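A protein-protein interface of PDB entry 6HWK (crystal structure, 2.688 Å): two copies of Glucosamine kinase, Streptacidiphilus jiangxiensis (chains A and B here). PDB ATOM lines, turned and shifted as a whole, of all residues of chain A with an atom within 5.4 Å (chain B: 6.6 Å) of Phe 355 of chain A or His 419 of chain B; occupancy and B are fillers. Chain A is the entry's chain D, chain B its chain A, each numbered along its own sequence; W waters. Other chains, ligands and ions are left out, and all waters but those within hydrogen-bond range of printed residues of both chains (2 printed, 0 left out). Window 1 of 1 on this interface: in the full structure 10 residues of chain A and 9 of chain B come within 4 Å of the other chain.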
ATOM      1  N   GLY A 350      10.767  25.621  -8.157  1.00  0.00           N
ATOM      2  CA  GLY A 350      11.840  25.785  -7.190  1.00  0.00           C
ATOM      3  C   GLY A 350      12.923  24.733  -7.331  1.00  0.00           C
ATOM      4  O   GLY A 350      14.113  25.034  -7.203  1.00  0.00           O
ATOM      5  N   ARG A 351      12.527  23.484  -7.596  1.00  0.00           N
ATOM      6  CA  ARG A 351      13.513  22.424  -7.794  1.00  0.00           C
ATOM      7  C   ARG A 351      14.367  22.694  -9.024  1.00  0.00           C
ATOM      8  O   ARG A 351      15.581  22.460  -9.013  1.00  0.00           O
ATOM      9  CB  ARG A 351      12.815  21.070  -7.925  1.00  0.00           C
ATOM     10  CG  ARG A 351      11.757  20.793  -6.870  1.00  0.00           C
ATOM     11  CD  ARG A 351      12.342  20.807  -5.472  1.00  0.00           C
ATOM     12  NE  ARG A 351      11.308  20.613  -4.460  1.00  0.00           N
ATOM     13  CZ  ARG A 351      11.541  20.582  -3.153  1.00  0.00           C
ATOM     14  NH1 ARG A 351      12.775  20.731  -2.693  1.00  0.00           N
ATOM     15  NH2 ARG A 351      10.538  20.401  -2.305  1.00  0.00           N
ATOM     16  N   VAL A 352      13.747  23.190 -10.096  1.00  0.00           N
ATOM     17  CA  VAL A 352      14.475  23.452 -11.334  1.00  0.00           C
ATOM     18  C   VAL A 352      15.458  24.603 -11.147  1.00  0.00           C
ATOM     19  O   VAL A 352      16.593  24.552 -11.635  1.00  0.00           O
ATOM     20  CB  VAL A 352      13.478  23.723 -12.476  1.00  0.00           C
ATOM     21  CG1 VAL A 352      14.157  24.431 -13.635  1.00  0.00           C
ATOM     22  CG2 VAL A 352      12.849  22.417 -12.941  1.00  0.00           C
ATOM     23  N   VAL A 353      15.044  25.651 -10.429  1.00  0.00           N
ATOM     24  CA  VAL A 353      15.922  26.799 -10.210  1.00  0.00           C
ATOM     25  C   VAL A 353      17.161  26.384  -9.425  1.00  0.00           C
ATOM     26  O   VAL A 353      18.284  26.784  -9.754  1.00  0.00           O
ATOM     27  CB  VAL A 353      15.152  27.933  -9.507  1.00  0.00           C
ATOM     28  CG1 VAL A 353      16.103  29.035  -9.065  1.00  0.00           C
ATOM     29  CG2 VAL A 353      14.087  28.498 -10.431  1.00  0.00           C
ATOM     30  N   VAL A 354      16.982  25.569  -8.383  1.00  0.00           N
ATOM     31  CA  VAL A 354      18.127  25.108  -7.604  1.00  0.00           C
ATOM     32  C   VAL A 354      18.991  24.153  -8.421  1.00  0.00           C
ATOM     33  O   VAL A 354      20.223  24.148  -8.290  1.00  0.00           O
ATOM     34  CB  VAL A 354      17.642  24.460  -6.292  1.00  0.00           C
ATOM     35  CG1 VAL A 354      18.774  23.709  -5.603  1.00  0.00           C
ATOM     36  CG2 VAL A 354      17.069  25.519  -5.366  1.00  0.00           C
ATOM     37  N   PHE A 355      18.373  23.357  -9.293  1.00  0.00           N
ATOM     38  CA  PHE A 355      19.099  22.321 -10.020  1.00  0.00           C
ATOM     39  C   PHE A 355      19.929  22.899 -11.162  1.00  0.00           C
ATOM     40  O   PHE A 355      21.037  22.420 -11.431  1.00  0.00           O
ATOM     41  CB  PHE A 355      18.106  21.286 -10.546  1.00  0.00           C
ATOM     42  CG  PHE A 355      18.745  20.096 -11.201  1.00  0.00           C
ATOM     43  CD1 PHE A 355      19.238  19.051 -10.439  1.00  0.00           C
ATOM     44  CD2 PHE A 355      18.823  20.008 -12.582  1.00  0.00           C
ATOM     45  CE1 PHE A 355      19.814  17.949 -11.039  1.00  0.00           C
ATOM     46  CE2 PHE A 355      19.397  18.909 -13.190  1.00  0.00           C
ATOM     47  CZ  PHE A 355      19.892  17.877 -12.416  1.00  0.00           C
ATOM     48  N   ARG A 356      19.420  23.930 -11.837  1.00  0.00           N
ATOM     49  CA  ARG A 356      20.044  24.433 -13.054  1.00  0.00           C
ATOM     50  C   ARG A 356      20.896  25.674 -12.846  1.00  0.00           C
ATOM     51  O   ARG A 356      21.809  25.920 -13.641  1.00  0.00           O
ATOM     52  CB  ARG A 356      18.975  24.748 -14.105  1.00  0.00           C
ATOM     53  CG  ARG A 356      18.145  23.554 -14.528  1.00  0.00           C
ATOM     54  CD  ARG A 356      17.128  23.956 -15.575  1.00  0.00           C
ATOM     55  NE  ARG A 356      16.275  22.839 -15.963  1.00  0.00           N
ATOM     56  CZ  ARG A 356      15.171  22.963 -16.692  1.00  0.00           C
ATOM     57  NH1 ARG A 356      14.783  24.161 -17.108  1.00  0.00           N
ATOM     58  NH2 ARG A 356      14.454  21.891 -16.999  1.00  0.00           N
ATOM     59  N   THR A 357      20.627  26.464 -11.815  1.00  0.00           N
ATOM     60  CA  THR A 357      21.330  27.731 -11.644  1.00  0.00           C
ATOM     61  C   THR A 357      22.663  27.503 -10.941  1.00  0.00           C
ATOM     62  O   THR A 357      22.681  26.959  -9.832  1.00  0.00           O
ATOM     63  CB  THR A 357      20.486  28.713 -10.844  1.00  0.00           C
ATOM     64  OG1 THR A 357      19.192  28.838 -11.447  1.00  0.00           O
ATOM     65  CG2 THR A 357      21.157  30.079 -10.802  1.00  0.00           C
ATOM     66  N   HIS A 419      16.751  11.936 -16.103  1.00  0.00           N
ATOM     67  CA  HIS A 419      17.273  12.642 -14.936  1.00  0.00           C
ATOM     68  C   HIS A 419      16.207  13.437 -14.195  1.00  0.00           C
ATOM     69  O   HIS A 419      16.506  13.996 -13.135  1.00  0.00           O
ATOM     70  CB  HIS A 419      18.418  13.575 -15.343  1.00  0.00           C
ATOM     71  CG  HIS A 419      17.966  14.917 -15.831  1.00  0.00           C
ATOM     72  ND1 HIS A 419      17.735  15.187 -17.163  1.00  0.00           N
ATOM     73  CD2 HIS A 419      17.720  16.072 -15.166  1.00  0.00           C
ATOM     74  CE1 HIS A 419      17.358  16.446 -17.296  1.00  0.00           C
ATOM     75  NE2 HIS A 419      17.339  17.005 -16.100  1.00  0.00           N
ATOM     76  N   TYR A 422      14.734  13.627 -10.038  1.00  0.00           N
ATOM     77  CA  TYR A 422      15.112  14.405  -8.862  1.00  0.00           C
ATOM     78  C   TYR A 422      13.971  15.293  -8.383  1.00  0.00           C
ATOM     79  O   TYR A 422      13.886  15.595  -7.188  1.00  0.00           O
ATOM     80  CB  TYR A 422      16.358  15.245  -9.155  1.00  0.00           C
ATOM     81  CG  TYR A 422      16.106  16.502  -9.964  1.00  0.00           C
ATOM     82  CD1 TYR A 422      16.101  16.470 -11.352  1.00  0.00           C
ATOM     83  CD2 TYR A 422      15.892  17.724  -9.339  1.00  0.00           C
ATOM     84  CE1 TYR A 422      15.879  17.616 -12.095  1.00  0.00           C
ATOM     85  CE2 TYR A 422      15.664  18.874 -10.072  1.00  0.00           C
ATOM     86  CZ  TYR A 422      15.661  18.815 -11.449  1.00  0.00           C
ATOM     87  OH  TYR A 422      15.439  19.959 -12.183  1.00  0.00           O
ATOM     88  N   PHE B 355      21.258  14.970 -22.252  1.00  0.00           N
ATOM     89  CA  PHE B 355      20.795  15.121 -20.878  1.00  0.00           C
ATOM     90  C   PHE B 355      19.533  15.969 -20.774  1.00  0.00           C
ATOM     91  O   PHE B 355      18.699  15.722 -19.896  1.00  0.00           O
ATOM     92  CB  PHE B 355      21.913  15.734 -20.033  1.00  0.00           C
ATOM     93  CG  PHE B 355      21.620  15.780 -18.563  1.00  0.00           C
ATOM     94  CD1 PHE B 355      21.899  14.693 -17.754  1.00  0.00           C
ATOM     95  CD2 PHE B 355      21.089  16.922 -17.982  1.00  0.00           C
ATOM     96  CE1 PHE B 355      21.641  14.737 -16.395  1.00  0.00           C
ATOM     97  CE2 PHE B 355      20.827  16.971 -16.625  1.00  0.00           C
ATOM     98  CZ  PHE B 355      21.106  15.879 -15.831  1.00  0.00           C
ATOM     99  N   ARG B 356      19.369  16.960 -21.651  1.00  0.00           N
ATOM    100  CA  ARG B 356      18.302  17.939 -21.496  1.00  0.00           C
ATOM    101  C   ARG B 356      17.141  17.750 -22.462  1.00  0.00           C
ATOM    102  O   ARG B 356      16.034  18.210 -22.163  1.00  0.00           O
ATOM    103  CB  ARG B 356      18.860  19.358 -21.666  1.00  0.00           C
ATOM    104  CG  ARG B 356      19.947  19.716 -20.670  1.00  0.00           C
ATOM    105  CD  ARG B 356      20.441  21.137 -20.875  1.00  0.00           C
ATOM    106  NE  ARG B 356      21.543  21.461 -19.974  1.00  0.00           N
ATOM    107  CZ  ARG B 356      22.244  22.589 -20.022  1.00  0.00           C
ATOM    108  NH1 ARG B 356      21.964  23.511 -20.934  1.00  0.00           N
ATOM    109  NH2 ARG B 356      23.229  22.795 -19.159  1.00  0.00           N
ATOM    110  N   ALA B 413      31.884  21.553 -11.173  1.00  0.00           N
ATOM    111  CA  ALA B 413      30.633  20.956 -10.719  1.00  0.00           C
ATOM    112  C   ALA B 413      30.505  21.023  -9.202  1.00  0.00           C
ATOM    113  O   ALA B 413      29.513  21.542  -8.676  1.00  0.00           O
ATOM    114  CB  ALA B 413      30.533  19.513 -11.210  1.00  0.00           C
ATOM    115  N   LEU B 417      27.924  23.912  -9.917  1.00  0.00           N
ATOM    116  CA  LEU B 417      26.752  23.184 -10.404  1.00  0.00           C
ATOM    117  C   LEU B 417      26.928  21.706 -10.082  1.00  0.00           C
ATOM    118  O   LEU B 417      27.517  20.954 -10.869  1.00  0.00           O
ATOM    119  CB  LEU B 417      26.552  23.407 -11.902  1.00  0.00           C
ATOM    120  CG  LEU B 417      25.163  23.114 -12.472  1.00  0.00           C
ATOM    121  CD1 LEU B 417      24.120  24.000 -11.812  1.00  0.00           C
ATOM    122  CD2 LEU B 417      25.156  23.306 -13.981  1.00  0.00           C
ATOM    123  N   PRO B 418      26.418  21.251  -8.932  1.00  0.00           N
ATOM    124  CA  PRO B 418      26.767  19.897  -8.459  1.00  0.00           C
ATOM    125  C   PRO B 418      26.401  18.775  -9.418  1.00  0.00           C
ATOM    126  O   PRO B 418      27.159  17.804  -9.537  1.00  0.00           O
ATOM    127  CB  PRO B 418      25.998  19.789  -7.135  1.00  0.00           C
ATOM    128  CG  PRO B 418      25.825  21.204  -6.683  1.00  0.00           C
ATOM    129  CD  PRO B 418      25.626  22.000  -7.942  1.00  0.00           C
ATOM    130  N   HIS B 419      25.267  18.872 -10.113  1.00  0.00           N
ATOM    131  CA  HIS B 419      24.867  17.780 -10.995  1.00  0.00           C
ATOM    132  C   HIS B 419      25.683  17.721 -12.280  1.00  0.00           C
ATOM    133  O   HIS B 419      25.504  16.777 -13.057  1.00  0.00           O
ATOM    134  CB  HIS B 419      23.376  17.889 -11.331  1.00  0.00           C
ATOM    135  CG  HIS B 419      23.078  18.764 -12.509  1.00  0.00           C
ATOM    136  ND1 HIS B 419      22.868  20.121 -12.395  1.00  0.00           N
ATOM    137  CD2 HIS B 419      22.943  18.472 -13.824  1.00  0.00           C
ATOM    138  CE1 HIS B 419      22.625  20.629 -13.591  1.00  0.00           C
ATOM    139  NE2 HIS B 419      22.665  19.650 -14.476  1.00  0.00           N
ATOM    140  N   TRP B 420      26.575  18.684 -12.518  1.00  0.00           N
ATOM    141  CA  TRP B 420      27.371  18.728 -13.739  1.00  0.00           C
ATOM    142  C   TRP B 420      28.417  17.618 -13.813  1.00  0.00           C
ATOM    143  O   TRP B 420      29.057  17.467 -14.859  1.00  0.00           O
ATOM    144  CB  TRP B 420      28.042  20.102 -13.855  1.00  0.00           C
ATOM    145  CG  TRP B 420      28.812  20.333 -15.121  1.00  0.00           C
ATOM    146  CD1 TRP B 420      30.169  20.340 -15.265  1.00  0.00           C
ATOM    147  CD2 TRP B 420      28.270  20.594 -16.421  1.00  0.00           C
ATOM    148  NE1 TRP B 420      30.505  20.589 -16.573  1.00  0.00           N
ATOM    149  CE2 TRP B 420      29.357  20.746 -17.304  1.00  0.00           C
ATOM    150  CE3 TRP B 420      26.971  20.711 -16.924  1.00  0.00           C
ATOM    151  CZ2 TRP B 420      29.185  21.010 -18.660  1.00  0.00           C
ATOM    152  CZ3 TRP B 420      26.803  20.975 -18.272  1.00  0.00           C
ATOM    153  CH2 TRP B 420      27.904  21.122 -19.124  1.00  0.00           C
ATOM    154  N   VAL B 421      28.591  16.828 -12.748  1.00  0.00           N
ATOM    155  CA  VAL B 421      29.606  15.778 -12.736  1.00  0.00           C
ATOM    156  C   VAL B 421      29.367  14.723 -13.808  1.00  0.00           C
ATOM    157  O   VAL B 421      30.290  13.980 -14.157  1.00  0.00           O
ATOM    158  CB  VAL B 421      29.681  15.111 -11.344  1.00  0.00           C
ATOM    159  CG1 VAL B 421      30.330  16.042 -10.331  1.00  0.00           C
ATOM    160  CG2 VAL B 421      28.293  14.694 -10.883  1.00  0.00           C
ATOM    161  N   TYR B 422      28.143  14.628 -14.339  1.00  0.00           N
ATOM    162  CA  TYR B 422      27.866  13.609 -15.347  1.00  0.00           C
ATOM    163  C   TYR B 422      28.609  13.887 -16.647  1.00  0.00           C
ATOM    164  O   TYR B 422      28.877  12.956 -17.415  1.00  0.00           O
ATOM    165  CB  TYR B 422      26.359  13.513 -15.610  1.00  0.00           C
ATOM    166  CG  TYR B 422      25.814  14.586 -16.532  1.00  0.00           C
ATOM    167  CD1 TYR B 422      25.402  15.814 -16.032  1.00  0.00           C
ATOM    168  CD2 TYR B 422      25.704  14.366 -17.902  1.00  0.00           C
ATOM    169  CE1 TYR B 422      24.904  16.795 -16.870  1.00  0.00           C
ATOM    170  CE2 TYR B 422      25.210  15.343 -18.746  1.00  0.00           C
ATOM    171  CZ  TYR B 422      24.810  16.554 -18.223  1.00  0.00           C
ATOM    172  OH  TYR B 422      24.317  17.529 -19.057  1.00  0.00           O
ATOM    173  N   VAL B 423      28.948  15.146 -16.911  1.00  0.00           N
ATOM    174  CA  VAL B 423      29.586  15.529 -18.170  1.00  0.00           C
ATOM    175  C   VAL B 423      31.006  14.970 -18.240  1.00  0.00           C
ATOM    176  O   VAL B 423      31.311  14.232 -19.188  1.00  0.00           O
ATOM    177  CB  VAL B 423      29.561  17.055 -18.367  1.00  0.00           C
ATOM    178  CG1 VAL B 423      30.316  17.432 -19.620  1.00  0.00           C
ATOM    179  CG2 VAL B 423      28.130  17.556 -18.437  1.00  0.00           C
HETATM  180  O   HOH W   1      18.471  12.898 -18.499  1.00  0.00           O
HETATM  181  O   HOH W   2      22.821  20.748  -9.606  1.00  0.00           O
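A ring nitrogen (ND1) of His 419 of chain A is in hydrogen-bond range of the backbone carbonyl oxygen (O) of Phe 355 of chain B (2.9 Å).
The backbone carbonyl oxygen (O) of Phe 355 of chain A is in hydrogen-bond range of a ring nitrogen (ND1) of His 419 of chain B, at 3.1 Å.
The side-chain hydroxyl (OG1) of Thr 357 of chain A sits at hydrogen-bond distance from the backbone carbonyl oxygen (O) of Val 353 of chain A (2.8 Å).
Among the printed residues, pairs that only touch across the chains: Phe 355 of chain A with Leu 417 of chain B, Arg 356 of chain A with Leu 417 of chain B and Thr 357 of chain A with Leu 417 of chain B.
Phe 355 of chain A touches just these residues of chain B: Leu 417 (3.5 Å) and His 419 (3.1 Å).
Of the printed residues of chain B, Arg 356 of chain A touches Leu 417 (3.5 Å).
Printed residues of chain B within 4 Å of Thr 357 of chain A: Leu 417 (3.8 Å).
Of the printed residues of chain B, His 419 of chain A touches Phe 355 (2.9 Å).
Of the printed residues of chain A, Phe 355 of chain B touches His 419.
Printed residues of chain A within 4 Å of Leu 417 of chain B: Phe 355 (3.5 Å), Arg 356 (3.5 Å) and Thr 357 (3.8 Å).
Trp 420 of chain B touches none of the printed residues of chain A.
The nearest residue of chain B that does not touch Phe 355 of chain A is Phe 355 of chain B (4.1 Å).
Hydrophobic or aromatic side chains of chain A that line the printed part of chain B: Phe 355 and His 419.
Of the 10 printed residues of chain B, 3 touch a printed residue of chain A.
Among the printed residues, no Asp or Glu carboxylate lies within 4 Å of a Lys or Arg side-chain nitrogen of the other chain.
Phe 355 of chain A touches His 419 of chain B, and with the chains exchanged His 419 of chain A touches Phe 355 of chain B.
4 positions are printed for both chains.
Of the 5 pairs that touch across the chains among the printed residues, 2 have their exchanged pair printed and touching as well.
Water W1 lies within hydrogen-bond range of a ring nitrogen (ND1) of His 419 of chain A and the backbone carbonyl oxygen (O) of Phe 355 of chain B.
Water W2 lies within hydrogen-bond range of a ring nitrogen (ND1) of His 419 of chain B and the backbone carbonyl oxygen (O) of Phe 355 of chain A.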
